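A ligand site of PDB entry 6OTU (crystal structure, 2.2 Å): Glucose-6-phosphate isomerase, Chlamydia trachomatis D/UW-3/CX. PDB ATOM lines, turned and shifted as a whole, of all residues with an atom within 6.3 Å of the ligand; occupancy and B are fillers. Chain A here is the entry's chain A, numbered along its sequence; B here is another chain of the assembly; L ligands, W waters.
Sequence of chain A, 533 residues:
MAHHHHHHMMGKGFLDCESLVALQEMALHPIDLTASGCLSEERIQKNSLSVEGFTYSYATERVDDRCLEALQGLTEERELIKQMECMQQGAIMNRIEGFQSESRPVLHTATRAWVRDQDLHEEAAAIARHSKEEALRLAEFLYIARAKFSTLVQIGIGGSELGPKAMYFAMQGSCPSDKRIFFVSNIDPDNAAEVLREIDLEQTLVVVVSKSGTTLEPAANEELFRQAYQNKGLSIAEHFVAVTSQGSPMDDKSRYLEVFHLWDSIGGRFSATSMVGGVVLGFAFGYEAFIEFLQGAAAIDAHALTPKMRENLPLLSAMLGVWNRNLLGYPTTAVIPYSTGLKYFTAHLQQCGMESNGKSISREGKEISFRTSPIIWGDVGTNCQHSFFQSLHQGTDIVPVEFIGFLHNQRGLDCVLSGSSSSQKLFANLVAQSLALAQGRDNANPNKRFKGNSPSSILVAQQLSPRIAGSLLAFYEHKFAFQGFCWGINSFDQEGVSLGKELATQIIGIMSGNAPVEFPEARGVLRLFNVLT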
ATOM      1  N   GLY A 156      17.214 -26.171 -16.078  1.00  0.00           N
ATOM      2  CA  GLY A 156      17.193 -24.817 -15.537  1.00  0.00           C
ATOM      3  C   GLY A 156      15.958 -24.107 -16.034  1.00  0.00           C
ATOM      4  O   GLY A 156      15.315 -24.521 -17.006  1.00  0.00           O
ATOM      5  N   ILE A 157      15.638 -23.005 -15.361  1.00  0.00           N
ATOM      6  CA  ILE A 157      14.391 -22.301 -15.642  1.00  0.00           C
ATOM      7  C   ILE A 157      14.649 -20.805 -15.610  1.00  0.00           C
ATOM      8  O   ILE A 157      15.649 -20.338 -15.045  1.00  0.00           O
ATOM      9  CB  ILE A 157      13.289 -22.723 -14.620  1.00  0.00           C
ATOM     10  CG1 ILE A 157      11.881 -22.309 -15.080  1.00  0.00           C
ATOM     11  CG2 ILE A 157      13.646 -22.226 -13.229  1.00  0.00           C
ATOM     12  CD1 ILE A 157      10.748 -22.970 -14.254  1.00  0.00           C
ATOM     13  N   GLY A 158      13.744 -20.047 -16.225  1.00  0.00           N
ATOM     14  CA  GLY A 158      13.843 -18.593 -16.171  1.00  0.00           C
ATOM     15  C   GLY A 158      15.113 -18.099 -16.840  1.00  0.00           C
ATOM     16  O   GLY A 158      15.450 -18.511 -17.961  1.00  0.00           O
ATOM     17  N   GLY A 159      15.850 -17.221 -16.150  1.00  0.00           N
ATOM     18  CA  GLY A 159      17.118 -16.729 -16.680  1.00  0.00           C
ATOM     19  C   GLY A 159      18.133 -17.826 -16.962  1.00  0.00           C
ATOM     20  O   GLY A 159      19.029 -17.626 -17.790  1.00  0.00           O
ATOM     21  N   SER A 160      18.017 -18.968 -16.301  1.00  0.00           N
ATOM     22  CA  SER A 160      18.910 -20.091 -16.548  1.00  0.00           C
ATOM     23  C   SER A 160      18.584 -20.887 -17.805  1.00  0.00           C
ATOM     24  O   SER A 160      19.371 -21.771 -18.152  1.00  0.00           O
ATOM     25  CB  SER A 160      18.937 -21.044 -15.333  1.00  0.00           C
ATOM     26  OG  SER A 160      19.497 -20.413 -14.183  1.00  0.00           O
ATOM     27  N   VAL A 209      21.804 -25.886 -14.354  1.00  0.00           N
ATOM     28  CA  VAL A 209      22.120 -24.473 -14.299  1.00  0.00           C
ATOM     29  C   VAL A 209      21.154 -23.833 -13.320  1.00  0.00           C
ATOM     30  O   VAL A 209      19.942 -23.784 -13.577  1.00  0.00           O
ATOM     31  CB  VAL A 209      22.044 -23.817 -15.692  1.00  0.00           C
ATOM     32  CG1 VAL A 209      22.363 -22.340 -15.597  1.00  0.00           C
ATOM     33  CG2 VAL A 209      22.965 -24.519 -16.686  1.00  0.00           C
ATOM     34  N   SER A 210      21.677 -23.357 -12.191  1.00  0.00           N
ATOM     35  CA  SER A 210      20.832 -22.688 -11.199  1.00  0.00           C
ATOM     36  C   SER A 210      21.725 -21.776 -10.376  1.00  0.00           C
ATOM     37  O   SER A 210      22.592 -22.270  -9.657  1.00  0.00           O
ATOM     38  CB  SER A 210      20.132 -23.718 -10.308  1.00  0.00           C
ATOM     39  OG  SER A 210      19.725 -23.125  -9.082  1.00  0.00           O
ATOM     40  N   LYS A 211      21.515 -20.460 -10.499  1.00  0.00           N
ATOM     41  CA  LYS A 211      22.355 -19.501  -9.785  1.00  0.00           C
ATOM     42  C   LYS A 211      22.295 -19.731  -8.282  1.00  0.00           C
ATOM     43  O   LYS A 211      23.327 -19.970  -7.643  1.00  0.00           O
ATOM     44  CB  LYS A 211      21.921 -18.062 -10.130  1.00  0.00           C
ATOM     45  CG  LYS A 211      22.654 -16.964  -9.355  1.00  0.00           C
ATOM     46  CD  LYS A 211      22.386 -15.550  -9.898  1.00  0.00           C
ATOM     47  CE  LYS A 211      22.874 -14.468  -8.930  1.00  0.00           C
ATOM     48  NZ  LYS A 211      22.538 -13.094  -9.379  1.00  0.00           N
ATOM     49  N   SER A 212      21.090 -19.705  -7.701  1.00  0.00           N
ATOM     50  CA  SER A 212      20.947 -19.944  -6.264  1.00  0.00           C
ATOM     51  C   SER A 212      21.403 -21.337  -5.866  1.00  0.00           C
ATOM     52  O   SER A 212      21.905 -21.525  -4.755  1.00  0.00           O
ATOM     53  CB  SER A 212      19.498 -19.752  -5.838  1.00  0.00           C
ATOM     54  OG  SER A 212      18.651 -20.692  -6.491  1.00  0.00           O
ATOM     55  N   GLY A 213      21.201 -22.328  -6.733  1.00  0.00           N
ATOM     56  CA  GLY A 213      21.339 -23.727  -6.360  1.00  0.00           C
ATOM     57  C   GLY A 213      20.176 -24.306  -5.581  1.00  0.00           C
ATOM     58  O   GLY A 213      20.298 -25.429  -5.076  1.00  0.00           O
ATOM     59  N   THR A 214      19.052 -23.577  -5.460  1.00  0.00           N
ATOM     60  CA  THR A 214      17.950 -24.037  -4.610  1.00  0.00           C
ATOM     61  C   THR A 214      16.556 -23.958  -5.258  1.00  0.00           C
ATOM     62  O   THR A 214      15.565 -24.265  -4.597  1.00  0.00           O
ATOM     63  CB  THR A 214      17.935 -23.250  -3.300  1.00  0.00           C
ATOM     64  OG1 THR A 214      17.951 -21.852  -3.589  1.00  0.00           O
ATOM     65  CG2 THR A 214      19.178 -23.577  -2.465  1.00  0.00           C
ATOM     66  N   THR A 215      16.458 -23.552  -6.527  1.00  0.00           N
ATOM     67  CA  THR A 215      15.150 -23.443  -7.175  1.00  0.00           C
ATOM     68  C   THR A 215      14.490 -24.815  -7.313  1.00  0.00           C
ATOM     69  O   THR A 215      15.137 -25.801  -7.681  1.00  0.00           O
ATOM     70  CB  THR A 215      15.315 -22.782  -8.539  1.00  0.00           C
ATOM     71  OG1 THR A 215      16.140 -21.620  -8.397  1.00  0.00           O
ATOM     72  CG2 THR A 215      13.951 -22.373  -9.096  1.00  0.00           C
ATOM     73  N   PRO A 218      14.848 -26.898 -11.242  1.00  0.00           N
ATOM     74  CA  PRO A 218      16.102 -27.631 -11.500  1.00  0.00           C
ATOM     75  C   PRO A 218      16.335 -28.773 -10.523  1.00  0.00           C
ATOM     76  O   PRO A 218      16.838 -29.827 -10.925  1.00  0.00           O
ATOM     77  CB  PRO A 218      17.184 -26.559 -11.348  1.00  0.00           C
ATOM     78  CG  PRO A 218      16.482 -25.260 -11.360  1.00  0.00           C
ATOM     79  CD  PRO A 218      15.082 -25.481 -10.940  1.00  0.00           C
ATOM     80  N   GLY A 267      22.876 -10.951 -12.914  1.00  0.00           N
ATOM     81  CA  GLY A 267      21.451 -11.238 -12.918  1.00  0.00           C
ATOM     82  C   GLY A 267      21.109 -12.368 -13.878  1.00  0.00           C
ATOM     83  O   GLY A 267      21.646 -12.462 -14.978  1.00  0.00           O
ATOM     84  N   GLY A 268      20.176 -13.234 -13.440  1.00  0.00           N
ATOM     85  CA  GLY A 268      19.788 -14.387 -14.245  1.00  0.00           C
ATOM     86  C   GLY A 268      19.378 -14.031 -15.656  1.00  0.00           C
ATOM     87  O   GLY A 268      19.828 -14.654 -16.623  1.00  0.00           O
ATOM     88  N   ARG A 269      18.514 -13.021 -15.799  1.00  0.00           N
ATOM     89  CA  ARG A 269      18.035 -12.584 -17.106  1.00  0.00           C
ATOM     90  C   ARG A 269      19.116 -11.838 -17.895  1.00  0.00           C
ATOM     91  O   ARG A 269      18.854 -11.404 -19.032  1.00  0.00           O
ATOM     92  CB  ARG A 269      16.791 -11.715 -16.950  1.00  0.00           C
ATOM     93  CG  ARG A 269      16.985 -10.481 -16.100  1.00  0.00           C
ATOM     94  CD  ARG A 269      15.658  -9.784 -15.827  1.00  0.00           C
ATOM     95  NE  ARG A 269      15.767  -8.755 -14.786  1.00  0.00           N
ATOM     96  CZ  ARG A 269      15.654  -8.981 -13.472  1.00  0.00           C
ATOM     97  NH1 ARG A 269      15.418 -10.201 -13.011  1.00  0.00           N
ATOM     98  NH2 ARG A 269      15.772  -7.980 -12.623  1.00  0.00           N
ATOM     99  N   PHE A 270      20.305 -11.671 -17.324  1.00  0.00           N
ATOM    100  CA  PHE A 270      21.438 -11.100 -18.022  1.00  0.00           C
ATOM    101  C   PHE A 270      22.626 -12.068 -18.067  1.00  0.00           C
ATOM    102  O   PHE A 270      23.758 -11.630 -18.255  1.00  0.00           O
ATOM    103  CB  PHE A 270      21.881  -9.785 -17.375  1.00  0.00           C
ATOM    104  CG  PHE A 270      20.779  -8.768 -17.207  1.00  0.00           C
ATOM    105  CD1 PHE A 270      20.423  -7.932 -18.240  1.00  0.00           C
ATOM    106  CD2 PHE A 270      20.114  -8.636 -15.995  1.00  0.00           C
ATOM    107  CE1 PHE A 270      19.423  -6.990 -18.081  1.00  0.00           C
ATOM    108  CE2 PHE A 270      19.114  -7.693 -15.836  1.00  0.00           C
ATOM    109  CZ  PHE A 270      18.780  -6.859 -16.881  1.00  0.00           C
ATOM    110  N   GLN A 351      11.065 -11.747 -21.049  1.00  0.00           N
ATOM    111  CA  GLN A 351      11.522 -11.892 -19.671  1.00  0.00           C
ATOM    112  C   GLN A 351      12.435 -10.736 -19.278  1.00  0.00           C
ATOM    113  O   GLN A 351      12.286 -10.144 -18.195  1.00  0.00           O
ATOM    114  CB  GLN A 351      12.262 -13.212 -19.470  1.00  0.00           C
ATOM    115  CG  GLN A 351      13.093 -13.171 -18.175  1.00  0.00           C
ATOM    116  CD  GLN A 351      13.680 -14.502 -17.777  1.00  0.00           C
ATOM    117  OE1 GLN A 351      14.155 -15.269 -18.614  1.00  0.00           O
ATOM    118  NE2 GLN A 351      13.656 -14.802 -16.472  1.00  0.00           N
ATOM    119  N   GLU A 355      10.557  -8.501 -16.646  1.00  0.00           N
ATOM    120  CA  GLU A 355      11.035  -8.793 -15.297  1.00  0.00           C
ATOM    121  C   GLU A 355      11.901  -7.659 -14.749  1.00  0.00           C
ATOM    122  O   GLU A 355      11.855  -7.348 -13.548  1.00  0.00           O
ATOM    123  CB  GLU A 355      11.799 -10.118 -15.279  1.00  0.00           C
ATOM    124  CG  GLU A 355      11.768 -10.792 -13.933  1.00  0.00           C
ATOM    125  CD  GLU A 355      12.806 -11.864 -13.823  1.00  0.00           C
ATOM    126  OE1 GLU A 355      12.964 -12.404 -12.718  1.00  0.00           O
ATOM    127  OE2 GLU A 355      13.473 -12.165 -14.835  1.00  0.00           O
ATOM    128  N   GLN A 494      13.854  -8.599  -8.400  1.00  0.00           N
ATOM    129  CA  GLN A 494      12.650  -9.273  -8.893  1.00  0.00           C
ATOM    130  C   GLN A 494      11.849  -9.835  -7.725  1.00  0.00           C
ATOM    131  O   GLN A 494      11.689 -11.049  -7.582  1.00  0.00           O
ATOM    132  CB  GLN A 494      13.012 -10.362  -9.913  1.00  0.00           C
ATOM    133  CG  GLN A 494      14.047 -11.403  -9.477  1.00  0.00           C
ATOM    134  CD  GLN A 494      15.475 -10.908  -9.466  1.00  0.00           C
ATOM    135  OE1 GLN A 494      15.950 -10.278 -10.404  1.00  0.00           O
ATOM    136  NE2 GLN A 494      16.192 -11.201  -8.370  1.00  0.00           N
ATOM    137  N   VAL A 497       9.270 -12.458  -8.474  1.00  0.00           N
ATOM    138  CA  VAL A 497       9.753 -13.814  -8.714  1.00  0.00           C
ATOM    139  C   VAL A 497      10.184 -14.480  -7.397  1.00  0.00           C
ATOM    140  O   VAL A 497       9.967 -15.678  -7.215  1.00  0.00           O
ATOM    141  CB  VAL A 497      10.898 -13.788  -9.730  1.00  0.00           C
ATOM    142  CG1 VAL A 497      11.504 -15.201  -9.893  1.00  0.00           C
ATOM    143  CG2 VAL A 497      10.411 -13.253 -11.073  1.00  0.00           C
ATOM    144  N   LYS A 501       8.765 -18.123  -5.888  1.00  0.00           N
ATOM    145  CA  LYS A 501       9.517 -19.209  -5.263  1.00  0.00           C
ATOM    146  C   LYS A 501       9.063 -19.442  -3.823  1.00  0.00           C
ATOM    147  O   LYS A 501       9.028 -20.587  -3.361  1.00  0.00           O
ATOM    148  CB  LYS A 501      11.014 -18.915  -5.316  1.00  0.00           C
ATOM    149  CG  LYS A 501      11.519 -18.667  -6.718  1.00  0.00           C
ATOM    150  CD  LYS A 501      13.026 -18.703  -6.739  1.00  0.00           C
ATOM    151  CE  LYS A 501      13.519 -18.529  -8.136  1.00  0.00           C
ATOM    152  NZ  LYS A 501      14.963 -18.835  -8.229  1.00  0.00           N
ATOM    153  N   HIS B 386       8.852 -17.247 -13.257  1.00  0.00           N
ATOM    154  CA  HIS B 386      10.226 -16.792 -13.103  1.00  0.00           C
ATOM    155  C   HIS B 386      10.566 -15.633 -14.018  1.00  0.00           C
ATOM    156  O   HIS B 386      11.717 -15.169 -14.015  1.00  0.00           O
ATOM    157  CB  HIS B 386      11.209 -17.950 -13.352  1.00  0.00           C
ATOM    158  CG  HIS B 386      10.939 -19.142 -12.500  1.00  0.00           C
ATOM    159  ND1 HIS B 386      11.704 -19.455 -11.390  1.00  0.00           N
ATOM    160  CD2 HIS B 386       9.982 -20.104 -12.575  1.00  0.00           C
ATOM    161  CE1 HIS B 386      11.238 -20.563 -10.834  1.00  0.00           C
ATOM    162  NE2 HIS B 386      10.180 -20.965 -11.519  1.00  0.00           N
ATOM    163  N   SER B 387       9.607 -15.153 -14.800  1.00  0.00           N
ATOM    164  CA  SER B 387       9.912 -14.138 -15.794  1.00  0.00           C
ATOM    165  C   SER B 387       8.911 -12.990 -15.738  1.00  0.00           C
ATOM    166  O   SER B 387       9.005 -12.142 -14.836  1.00  0.00           O
ATOM    167  CB  SER B 387       9.981 -14.757 -17.204  1.00  0.00           C
ATOM    168  OG  SER B 387       8.715 -15.120 -17.677  1.00  0.00           O
HETATM  169  C1  LIG L   1      16.246 -14.015 -13.431  1.00  0.00           C
HETATM  170  C2  LIG L   1      15.186 -14.450 -12.425  1.00  0.00           C
HETATM  171  C3  LIG L   1      14.694 -15.873 -12.617  1.00  0.00           C
HETATM  172  C4  LIG L   1      15.728 -16.951 -12.254  1.00  0.00           C
HETATM  173  C5  LIG L   1      15.078 -18.324 -12.131  1.00  0.00           C
HETATM  174  C6  LIG L   1      16.099 -19.428 -11.947  1.00  0.00           C
HETATM  175  O1  LIG L   1      16.802 -12.977 -13.278  1.00  0.00           O
HETATM  176  O2  LIG L   1      15.646 -14.290 -11.086  1.00  0.00           O
HETATM  177  O3  LIG L   1      14.282 -16.060 -13.975  1.00  0.00           O
HETATM  178  O4  LIG L   1      16.754 -17.005 -13.245  1.00  0.00           O
HETATM  179  O5  LIG L   1      14.153 -18.314 -11.035  1.00  0.00           O
HETATM  180  O6  LIG L   1      16.897 -19.105 -10.786  1.00  0.00           O
HETATM  181  P1  LIG L   1      18.218 -19.985 -10.451  1.00  0.00           P
HETATM  182  O7  LIG L   1      19.176 -19.784 -11.605  1.00  0.00           O
HETATM  183  O8  LIG L   1      18.737 -19.401  -9.141  1.00  0.00           O
HETATM  184  O9  LIG L   1      17.762 -21.426 -10.307  1.00  0.00           O
HETATM  185  O   HOH W   1      18.391 -15.426 -10.743  1.00  0.00           O
HETATM  186  O   HOH W   2      18.167 -11.163 -11.529  1.00  0.00           O
HETATM  187  O   HOH W   3      17.430 -22.760 -12.909  1.00  0.00           O
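The side-chain hydroxyl of Thr 215 is in hydrogen-bond range of an oxygen (O9) of the ligand (2.5 Å). O7 of the ligand sits at hydrogen-bond distance from OG of Ser 160, 2.7 Å away. An oxygen (O7) of the ligand lies within hydrogen-bond range of the backbone NH of Lys 211 (2.7 Å). O3 of the ligand lies within hydrogen-bond range of O of His 386 of chain B, at 2.7 Å. ND1 of His 386 of chain B sits at hydrogen-bond distance from O5 of the ligand. The backbone NH (N) of Ser 212 sits at hydrogen-bond distance from an oxygen (O8) of the ligand, 2.8 Å away. OG of Ser 212 sits at hydrogen-bond distance from O8 of the ligand (2.9 Å). NE2 of Gln 351 is in hydrogen-bond range of O3 of the ligand (2.9 Å). The side-chain hydroxyl (OG) of Ser 210 lies within hydrogen-bond range of an oxygen (O9) of the ligand (2.9 Å). The backbone NH (N) of Gly 159 sits at hydrogen-bond distance from an oxygen (O3) of the ligand, 2.9 Å away. NZ of Lys 501 lies within salt-bridge range of O8 of the ligand, 3.9 Å away. The backbone NH (N) of Arg 269 lies within hydrogen-bond range of an oxygen (O1) of the ligand, at 3.0 Å. NH1 of Arg 269 sits at hydrogen-bond distance from O1 of the ligand (3.1 Å). O1 of the ligand is in hydrogen-bond range of N of Gly 268.
The side-chain hydroxyl (OG) of Ser 212 sits at hydrogen-bond distance from the side-chain hydroxyl (OG1) of Thr 215 (3.3 Å). The side-chain amino group (NZ) of Lys 501 lies within hydrogen-bond range of the side-chain hydroxyl (OG1) of Thr 215 (3.0 Å). The backbone carbonyl oxygen of Val 209 sits close to the side-chain hydroxyl of Ser 160 (3.5 Å). The side-chain hydroxyl of Ser 212 lies within hydrogen-bond range of the backbone NH of Thr 214 (3.1 Å). The backbone NH (N) of Gly 159 lies close to the side-chain amide nitrogen (NE2) of Gln 351, 3.3 Å away. The side-chain amide nitrogen (NE2) of Gln 351 lies within hydrogen-bond range of the side-chain carboxylate (OE2) of Glu 355, at 3.1 Å. The backbone NH (N) of Gly 213 is in hydrogen-bond range of the side-chain hydroxyl (OG) of Ser 210 (2.9 Å). OE1 of Glu 355 lies within salt-bridge range of NH1 of Arg 269 (3.3 Å).
Ile 157 touches the ligand (O to C6, 3.3 Å). CA of Gly 158 touches O3 of the ligand, 3.4 Å away. Glu 355 touches the ligand (OE1 to C2, 3.0 Å). Gln 494 touches the ligand. Of the 24 residues printed, 15 come within 4 Å of the ligand.
Water W2 lies within hydrogen-bond range of the side-chain amide oxygen of Gln 494, an oxygen (O1) of the ligand, the guanidinium group of Arg 269 and the backbone NH of Gly 268. Water W3 lies within hydrogen-bond range of the backbone carbonyl oxygen of Val 209, an oxygen (O9) of the ligand, the backbone NH of Ile 157 and the side-chain hydroxyl of Ser 160.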
